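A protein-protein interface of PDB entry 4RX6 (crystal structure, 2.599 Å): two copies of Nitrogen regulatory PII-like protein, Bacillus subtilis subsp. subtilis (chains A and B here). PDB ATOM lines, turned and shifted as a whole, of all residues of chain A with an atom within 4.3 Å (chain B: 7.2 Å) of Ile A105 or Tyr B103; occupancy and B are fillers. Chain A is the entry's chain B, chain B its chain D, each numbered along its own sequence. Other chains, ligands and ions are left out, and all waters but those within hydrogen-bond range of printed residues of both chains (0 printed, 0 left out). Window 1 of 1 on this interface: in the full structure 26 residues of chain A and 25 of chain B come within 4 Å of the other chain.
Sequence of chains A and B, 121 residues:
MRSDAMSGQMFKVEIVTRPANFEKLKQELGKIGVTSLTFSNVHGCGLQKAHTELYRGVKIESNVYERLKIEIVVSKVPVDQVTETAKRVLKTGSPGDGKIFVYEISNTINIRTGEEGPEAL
The side-chain amino group of Lys A12 lies within salt-bridge range of the side-chain carboxylate of Glu B14 (2.9 Å).
N of Ser A106 sits at hydrogen-bond distance from O of Val B102, 3.0 Å away.
The backbone NH (N) of Val B102 is in hydrogen-bond range of the backbone carbonyl oxygen (O) of Asn A107 (3.1 Å).
The backbone carbonyl oxygen (O) of Met A10 sits at hydrogen-bond distance from the backbone NH (N) of Ile A105 (3.0 Å).
OG1 of Thr A108 sits close to SD of Met A10, 3.4 Å away.
O of Tyr A103 lies within hydrogen-bond range of N of Lys A12.
O of Tyr B103 is in hydrogen-bond range of N of Lys B12, at 2.9 Å.
The side-chain carboxylate (OE1) of Glu B14 lies within salt-bridge range of the side-chain amino group (NZ) of Lys B69 (3.5 Å).
N of Glu B14 sits at hydrogen-bond distance from O of Phe B101, 2.7 Å away.
Among the printed residues, pairs that only touch across the chains: Thr A108 with Ile B100, Ile A105 with Tyr B103, Glu A104 with Tyr B103, Ile A105 with Val B102, Asn A107 with Phe B101, Asn A107 with Ile B100, Thr A108 with Phe B101 and Ser A106 with Tyr B103.
Ile A105 touches just these residues of chain B: Val B102 (3.5 Å) and Tyr B103 (3.5 Å).
Printed residues of chain B within 4 Å of Asn A107: Ile B100 (3.7 Å), Phe B101 (3.6 Å) and Val B102 (3.1 Å).
Of the printed residues of chain B, Thr A108 touches Ile B100 (3.2 Å) and Phe B101 (3.7 Å).
Glu B71 touches none of the printed residues of chain A.
Of the printed residues of chain A, Tyr B103 touches Glu A104 (3.5 Å), Ile A105 (3.5 Å) and Ser A106 (3.9 Å).
The nearest residue of chain A that does not touch Tyr B103 is Tyr A103 (4.1 Å).
The nearest printed residue of chain B that does not touch Asn A107 is Tyr B103 (5.4 Å).
Of the 14 printed residues of chain B, 5 touch a printed residue of chain A.
Printed residues of chain A that touch a printed residue of chain B: Lys A12, Glu A104, Ile A105, Ser A106, Asn A107 and Thr A108.
Among the printed residues, 11 pairs touch across the chains.
Glu A104 touches Tyr B103, but with the chains exchanged Tyr A103 does not touch Glu B104 (7.1 Å).
Ile A105 touches Tyr B103, but with the chains exchanged Tyr A103 does not touch Ile B105 (8.0 Å).
Of the 11 pairs that touch across the chains among the printed residues, none has its exchanged pair printed and touching as well.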
ATOM      1  N   MET A  10      14.786  10.227  31.659  1.00  0.00           N
ATOM      2  CA  MET A  10      13.607   9.385  31.685  1.00  0.00           C
ATOM      3  C   MET A  10      13.797   8.329  32.766  1.00  0.00           C
ATOM      4  O   MET A  10      14.912   7.873  33.002  1.00  0.00           O
ATOM      5  CB  MET A  10      13.430   8.758  30.314  1.00  0.00           C
ATOM      6  CG  MET A  10      14.373   9.383  29.295  1.00  0.00           C
ATOM      7  SD  MET A  10      14.032   8.895  27.614  1.00  0.00           S
ATOM      8  CE  MET A  10      12.268   9.156  27.628  1.00  0.00           C
ATOM      9  N   PHE A  11      12.720   7.972  33.456  1.00  0.00           N
ATOM     10  CA  PHE A  11      12.812   7.006  34.548  1.00  0.00           C
ATOM     11  C   PHE A  11      11.687   6.009  34.499  1.00  0.00           C
ATOM     12  O   PHE A  11      10.591   6.299  33.998  1.00  0.00           O
ATOM     13  CB  PHE A  11      12.789   7.691  35.908  1.00  0.00           C
ATOM     14  CG  PHE A  11      14.013   8.490  36.193  1.00  0.00           C
ATOM     15  CD1 PHE A  11      15.064   7.937  36.917  1.00  0.00           C
ATOM     16  CD2 PHE A  11      14.124   9.798  35.733  1.00  0.00           C
ATOM     17  CE1 PHE A  11      16.201   8.681  37.182  1.00  0.00           C
ATOM     18  CE2 PHE A  11      15.259  10.543  35.993  1.00  0.00           C
ATOM     19  CZ  PHE A  11      16.298   9.983  36.716  1.00  0.00           C
ATOM     20  N   LYS A  12      11.977   4.819  35.013  1.00  0.00           N
ATOM     21  CA  LYS A  12      10.957   3.817  35.172  1.00  0.00           C
ATOM     22  C   LYS A  12      10.653   3.665  36.634  1.00  0.00           C
ATOM     23  O   LYS A  12      11.551   3.539  37.467  1.00  0.00           O
ATOM     24  CB  LYS A  12      11.413   2.482  34.613  1.00  0.00           C
ATOM     25  CG  LYS A  12      10.657   1.295  35.195  1.00  0.00           C
ATOM     26  CD  LYS A  12       9.896   0.584  34.136  1.00  0.00           C
ATOM     27  CE  LYS A  12      10.684  -0.595  33.661  1.00  0.00           C
ATOM     28  NZ  LYS A  12      10.646  -0.710  32.214  1.00  0.00           N
ATOM     29  N   TYR A 103      14.506   3.119  38.495  1.00  0.00           N
ATOM     30  CA  TYR A 103      15.785   3.079  37.799  1.00  0.00           C
ATOM     31  C   TYR A 103      15.703   3.869  36.506  1.00  0.00           C
ATOM     32  O   TYR A 103      14.614   4.223  36.062  1.00  0.00           O
ATOM     33  CB  TYR A 103      16.265   1.637  37.547  1.00  0.00           C
ATOM     34  CG  TYR A 103      15.272   0.679  36.890  1.00  0.00           C
ATOM     35  CD1 TYR A 103      15.260   0.478  35.513  1.00  0.00           C
ATOM     36  CD2 TYR A 103      14.376  -0.053  37.658  1.00  0.00           C
ATOM     37  CE1 TYR A 103      14.367  -0.406  34.926  1.00  0.00           C
ATOM     38  CE2 TYR A 103      13.488  -0.930  37.080  1.00  0.00           C
ATOM     39  CZ  TYR A 103      13.489  -1.101  35.724  1.00  0.00           C
ATOM     40  OH  TYR A 103      12.596  -1.992  35.190  1.00  0.00           O
ATOM     41  N   GLU A 104      16.843   4.165  35.893  1.00  0.00           N
ATOM     42  CA  GLU A 104      16.806   5.109  34.787  1.00  0.00           C
ATOM     43  C   GLU A 104      16.874   4.501  33.391  1.00  0.00           C
ATOM     44  O   GLU A 104      17.532   3.505  33.144  1.00  0.00           O
ATOM     45  CB  GLU A 104      17.847   6.211  34.949  1.00  0.00           C
ATOM     46  CG  GLU A 104      19.258   5.767  35.130  1.00  0.00           C
ATOM     47  CD  GLU A 104      20.198   6.977  35.161  1.00  0.00           C
ATOM     48  OE1 GLU A 104      19.885   7.991  34.466  1.00  0.00           O
ATOM     49  OE2 GLU A 104      21.224   6.921  35.893  1.00  0.00           O
ATOM     50  N   ILE A 105      16.190   5.174  32.482  1.00  0.00           N
ATOM     51  CA  ILE A 105      15.996   4.720  31.131  1.00  0.00           C
ATOM     52  C   ILE A 105      16.881   5.560  30.203  1.00  0.00           C
ATOM     53  O   ILE A 105      16.731   6.786  30.135  1.00  0.00           O
ATOM     54  CB  ILE A 105      14.474   4.827  30.784  1.00  0.00           C
ATOM     55  CG1 ILE A 105      13.690   3.834  31.640  1.00  0.00           C
ATOM     56  CG2 ILE A 105      14.194   4.561  29.338  1.00  0.00           C
ATOM     57  CD1 ILE A 105      14.171   2.409  31.502  1.00  0.00           C
ATOM     58  N   SER A 106      17.814   4.896  29.519  1.00  0.00           N
ATOM     59  CA  SER A 106      18.649   5.531  28.507  1.00  0.00           C
ATOM     60  C   SER A 106      17.836   6.090  27.364  1.00  0.00           C
ATOM     61  O   SER A 106      18.168   7.143  26.836  1.00  0.00           O
ATOM     62  CB  SER A 106      19.630   4.537  27.899  1.00  0.00           C
ATOM     63  OG  SER A 106      20.409   3.916  28.897  1.00  0.00           O
ATOM     64  N   ASN A 107      16.795   5.379  26.946  1.00  0.00           N
ATOM     65  CA  ASN A 107      16.045   5.842  25.800  1.00  0.00           C
ATOM     66  C   ASN A 107      14.615   5.323  25.751  1.00  0.00           C
ATOM     67  O   ASN A 107      14.331   4.240  26.248  1.00  0.00           O
ATOM     68  CB  ASN A 107      16.790   5.434  24.528  1.00  0.00           C
ATOM     69  CG  ASN A 107      16.315   6.188  23.297  1.00  0.00           C
ATOM     70  OD1 ASN A 107      15.797   7.308  23.395  1.00  0.00           O
ATOM     71  ND2 ASN A 107      16.486   5.571  22.127  1.00  0.00           N
ATOM     72  N   THR A 108      13.716   6.095  25.146  1.00  0.00           N
ATOM     73  CA  THR A 108      12.362   5.616  24.889  1.00  0.00           C
ATOM     74  C   THR A 108      12.061   5.808  23.404  1.00  0.00           C
ATOM     75  O   THR A 108      12.423   6.828  22.831  1.00  0.00           O
ATOM     76  CB  THR A 108      11.319   6.353  25.766  1.00  0.00           C
ATOM     77  OG1 THR A 108      11.749   6.354  27.133  1.00  0.00           O
ATOM     78  CG2 THR A 108       9.970   5.677  25.689  1.00  0.00           C
ATOM     79  N   MET B  10      26.626  -3.395  27.814  1.00  0.00           N
ATOM     80  CA  MET B  10      25.483  -4.272  27.567  1.00  0.00           C
ATOM     81  C   MET B  10      24.197  -3.506  27.875  1.00  0.00           C
ATOM     82  O   MET B  10      24.153  -2.718  28.813  1.00  0.00           O
ATOM     83  CB  MET B  10      25.590  -5.515  28.438  1.00  0.00           C
ATOM     84  CG  MET B  10      27.026  -5.880  28.744  1.00  0.00           C
ATOM     85  SD  MET B  10      27.239  -7.097  30.056  1.00  0.00           S
ATOM     86  CE  MET B  10      26.669  -8.538  29.154  1.00  0.00           C
ATOM     87  N   PHE B  11      23.166  -3.706  27.061  1.00  0.00           N
ATOM     88  CA  PHE B  11      21.903  -3.005  27.231  1.00  0.00           C
ATOM     89  C   PHE B  11      20.736  -3.968  27.114  1.00  0.00           C
ATOM     90  O   PHE B  11      20.775  -4.930  26.337  1.00  0.00           O
ATOM     91  CB  PHE B  11      21.730  -1.942  26.158  1.00  0.00           C
ATOM     92  CG  PHE B  11      22.742  -0.853  26.216  1.00  0.00           C
ATOM     93  CD1 PHE B  11      24.034  -1.063  25.760  1.00  0.00           C
ATOM     94  CD2 PHE B  11      22.400   0.395  26.696  1.00  0.00           C
ATOM     95  CE1 PHE B  11      24.969  -0.049  25.806  1.00  0.00           C
ATOM     96  CE2 PHE B  11      23.335   1.412  26.743  1.00  0.00           C
ATOM     97  CZ  PHE B  11      24.618   1.190  26.295  1.00  0.00           C
ATOM     98  N   LYS B  12      19.689  -3.686  27.877  1.00  0.00           N
ATOM     99  CA  LYS B  12      18.435  -4.401  27.767  1.00  0.00           C
ATOM    100  C   LYS B  12      17.504  -3.540  26.936  1.00  0.00           C
ATOM    101  O   LYS B  12      17.460  -2.334  27.131  1.00  0.00           O
ATOM    102  CB  LYS B  12      17.845  -4.591  29.154  1.00  0.00           C
ATOM    103  CG  LYS B  12      16.392  -4.996  29.159  1.00  0.00           C
ATOM    104  CD  LYS B  12      16.272  -6.485  29.107  1.00  0.00           C
ATOM    105  CE  LYS B  12      15.317  -6.984  30.179  1.00  0.00           C
ATOM    106  NZ  LYS B  12      15.776  -6.685  31.544  1.00  0.00           N
ATOM    107  N   VAL B  13      16.782  -4.145  25.999  1.00  0.00           N
ATOM    108  CA  VAL B  13      15.774  -3.431  25.225  1.00  0.00           C
ATOM    109  C   VAL B  13      14.440  -4.073  25.528  1.00  0.00           C
ATOM    110  O   VAL B  13      14.306  -5.291  25.493  1.00  0.00           O
ATOM    111  CB  VAL B  13      15.994  -3.511  23.698  1.00  0.00           C
ATOM    112  CG1 VAL B  13      17.455  -3.432  23.345  1.00  0.00           C
ATOM    113  CG2 VAL B  13      15.402  -4.775  23.165  1.00  0.00           C
ATOM    114  N   GLU B  14      13.443  -3.255  25.807  1.00  0.00           N
ATOM    115  CA  GLU B  14      12.192  -3.755  26.321  1.00  0.00           C
ATOM    116  C   GLU B  14      11.147  -3.258  25.363  1.00  0.00           C
ATOM    117  O   GLU B  14      10.996  -2.060  25.183  1.00  0.00           O
ATOM    118  CB  GLU B  14      11.960  -3.197  27.718  1.00  0.00           C
ATOM    119  CG  GLU B  14      11.075  -4.048  28.586  1.00  0.00           C
ATOM    120  CD  GLU B  14      11.132  -3.656  30.059  1.00  0.00           C
ATOM    121  OE1 GLU B  14      10.140  -3.062  30.547  1.00  0.00           O
ATOM    122  OE2 GLU B  14      12.166  -3.944  30.717  1.00  0.00           O
ATOM    123  N   LYS B  69       5.449  -8.356  26.002  1.00  0.00           N
ATOM    124  CA  LYS B  69       6.671  -7.761  26.507  1.00  0.00           C
ATOM    125  C   LYS B  69       7.863  -8.590  26.080  1.00  0.00           C
ATOM    126  O   LYS B  69       8.064  -9.700  26.568  1.00  0.00           O
ATOM    127  CB  LYS B  69       6.641  -7.672  28.017  1.00  0.00           C
ATOM    128  CG  LYS B  69       7.826  -6.952  28.616  1.00  0.00           C
ATOM    129  CD  LYS B  69       7.571  -6.687  30.080  1.00  0.00           C
ATOM    130  CE  LYS B  69       8.464  -5.608  30.618  1.00  0.00           C
ATOM    131  NZ  LYS B  69       8.725  -5.838  32.066  1.00  0.00           N
ATOM    132  N   GLU B  71      11.984  -8.859  25.731  1.00  0.00           N
ATOM    133  CA  GLU B  71      13.192  -8.303  26.330  1.00  0.00           C
ATOM    134  C   GLU B  71      14.413  -8.949  25.703  1.00  0.00           C
ATOM    135  O   GLU B  71      14.626 -10.139  25.834  1.00  0.00           O
ATOM    136  CB  GLU B  71      13.200  -8.499  27.845  1.00  0.00           C
ATOM    137  CG  GLU B  71      11.832  -8.813  28.408  1.00  0.00           C
ATOM    138  CD  GLU B  71      11.778  -8.884  29.934  1.00  0.00           C
ATOM    139  OE1 GLU B  71      10.863  -9.573  30.447  1.00  0.00           O
ATOM    140  OE2 GLU B  71      12.619  -8.256  30.621  1.00  0.00           O
ATOM    141  N   VAL B  79      22.997  -1.962  19.916  1.00  0.00           N
ATOM    142  CA  VAL B  79      21.670  -1.592  20.369  1.00  0.00           C
ATOM    143  C   VAL B  79      20.926  -0.887  19.259  1.00  0.00           C
ATOM    144  O   VAL B  79      19.782  -1.224  18.946  1.00  0.00           O
ATOM    145  CB  VAL B  79      21.718  -0.578  21.511  1.00  0.00           C
ATOM    146  CG1 VAL B  79      20.311  -0.275  21.989  1.00  0.00           C
ATOM    147  CG2 VAL B  79      22.576  -1.074  22.648  1.00  0.00           C
ATOM    148  N   ILE B 100       9.281   1.395  23.192  1.00  0.00           N
ATOM    149  CA  ILE B 100      10.520   0.662  23.423  1.00  0.00           C
ATOM    150  C   ILE B 100      11.364   1.342  24.503  1.00  0.00           C
ATOM    151  O   ILE B 100      11.680   2.520  24.393  1.00  0.00           O
ATOM    152  CB  ILE B 100      11.346   0.582  22.138  1.00  0.00           C
ATOM    153  CG1 ILE B 100      10.539  -0.105  21.040  1.00  0.00           C
ATOM    154  CG2 ILE B 100      12.668  -0.130  22.388  1.00  0.00           C
ATOM    155  CD1 ILE B 100      11.247  -0.130  19.688  1.00  0.00           C
ATOM    156  N   PHE B 101      11.717   0.600  25.547  1.00  0.00           N
ATOM    157  CA  PHE B 101      12.452   1.163  26.669  1.00  0.00           C
ATOM    158  C   PHE B 101      13.803   0.490  26.714  1.00  0.00           C
ATOM    159  O   PHE B 101      13.878  -0.734  26.714  1.00  0.00           O
ATOM    160  CB  PHE B 101      11.700   0.924  27.977  1.00  0.00           C
ATOM    161  CG  PHE B 101      10.235   1.290  27.919  1.00  0.00           C
ATOM    162  CD1 PHE B 101       9.839   2.608  27.819  1.00  0.00           C
ATOM    163  CD2 PHE B 101       9.257   0.313  27.994  1.00  0.00           C
ATOM    164  CE1 PHE B 101       8.509   2.944  27.776  1.00  0.00           C
ATOM    165  CE2 PHE B 101       7.928   0.643  27.960  1.00  0.00           C
ATOM    166  CZ  PHE B 101       7.553   1.960  27.850  1.00  0.00           C
ATOM    167  N   VAL B 102      14.869   1.278  26.738  1.00  0.00           N
ATOM    168  CA  VAL B 102      16.224   0.738  26.756  1.00  0.00           C
ATOM    169  C   VAL B 102      16.916   1.183  28.028  1.00  0.00           C
ATOM    170  O   VAL B 102      16.796   2.331  28.415  1.00  0.00           O
ATOM    171  CB  VAL B 102      17.040   1.267  25.552  1.00  0.00           C
ATOM    172  CG1 VAL B 102      18.497   0.837  25.647  1.00  0.00           C
ATOM    173  CG2 VAL B 102      16.423   0.804  24.232  1.00  0.00           C
ATOM    174  N   TYR B 103      17.627   0.294  28.701  1.00  0.00           N
ATOM    175  CA  TYR B 103      18.454   0.726  29.822  1.00  0.00           C
ATOM    176  C   TYR B 103      19.743  -0.069  29.866  1.00  0.00           C
ATOM    177  O   TYR B 103      19.912  -1.029  29.125  1.00  0.00           O
ATOM    178  CB  TYR B 103      17.707   0.646  31.154  1.00  0.00           C
ATOM    179  CG  TYR B 103      16.877  -0.602  31.379  1.00  0.00           C
ATOM    180  CD1 TYR B 103      17.374  -1.666  32.125  1.00  0.00           C
ATOM    181  CD2 TYR B 103      15.583  -0.702  30.870  1.00  0.00           C
ATOM    182  CE1 TYR B 103      16.608  -2.801  32.348  1.00  0.00           C
ATOM    183  CE2 TYR B 103      14.814  -1.823  31.085  1.00  0.00           C
ATOM    184  CZ  TYR B 103      15.330  -2.871  31.822  1.00  0.00           C
ATOM    185  OH  TYR B 103      14.560  -3.993  32.035  1.00  0.00           O
ATOM    186  N   GLU B 104      20.662   0.342  30.727  1.00  0.00           N
ATOM    187  CA  GLU B 104      21.993  -0.236  30.717  1.00  0.00           C
ATOM    188  C   GLU B 104      22.130  -1.329  31.777  1.00  0.00           C
ATOM    189  O   GLU B 104      21.594  -1.210  32.880  1.00  0.00           O
ATOM    190  CB  GLU B 104      23.037   0.859  30.923  1.00  0.00           C
ATOM    191  CG  GLU B 104      24.463   0.364  30.856  1.00  0.00           C
ATOM    192  CD  GLU B 104      25.466   1.491  31.052  1.00  0.00           C
ATOM    193  OE1 GLU B 104      25.032   2.618  31.408  1.00  0.00           O
ATOM    194  OE2 GLU B 104      26.681   1.245  30.850  1.00  0.00           O
ATOM    195  N   ILE B 105      22.853  -2.385  31.423  1.00  0.00           N
ATOM    196  CA  ILE B 105      23.043  -3.558  32.263  1.00  0.00           C
ATOM    197  C   ILE B 105      24.478  -3.589  32.791  1.00  0.00           C
ATOM    198  O   ILE B 105      25.429  -3.424  32.023  1.00  0.00           O
ATOM    199  CB  ILE B 105      22.778  -4.840  31.434  1.00  0.00           C
ATOM    200  CG1 ILE B 105      21.304  -4.899  30.994  1.00  0.00           C
ATOM    201  CG2 ILE B 105      23.157  -6.087  32.207  1.00  0.00           C
ATOM    202  CD1 ILE B 105      20.309  -5.050  32.139  1.00  0.00           C
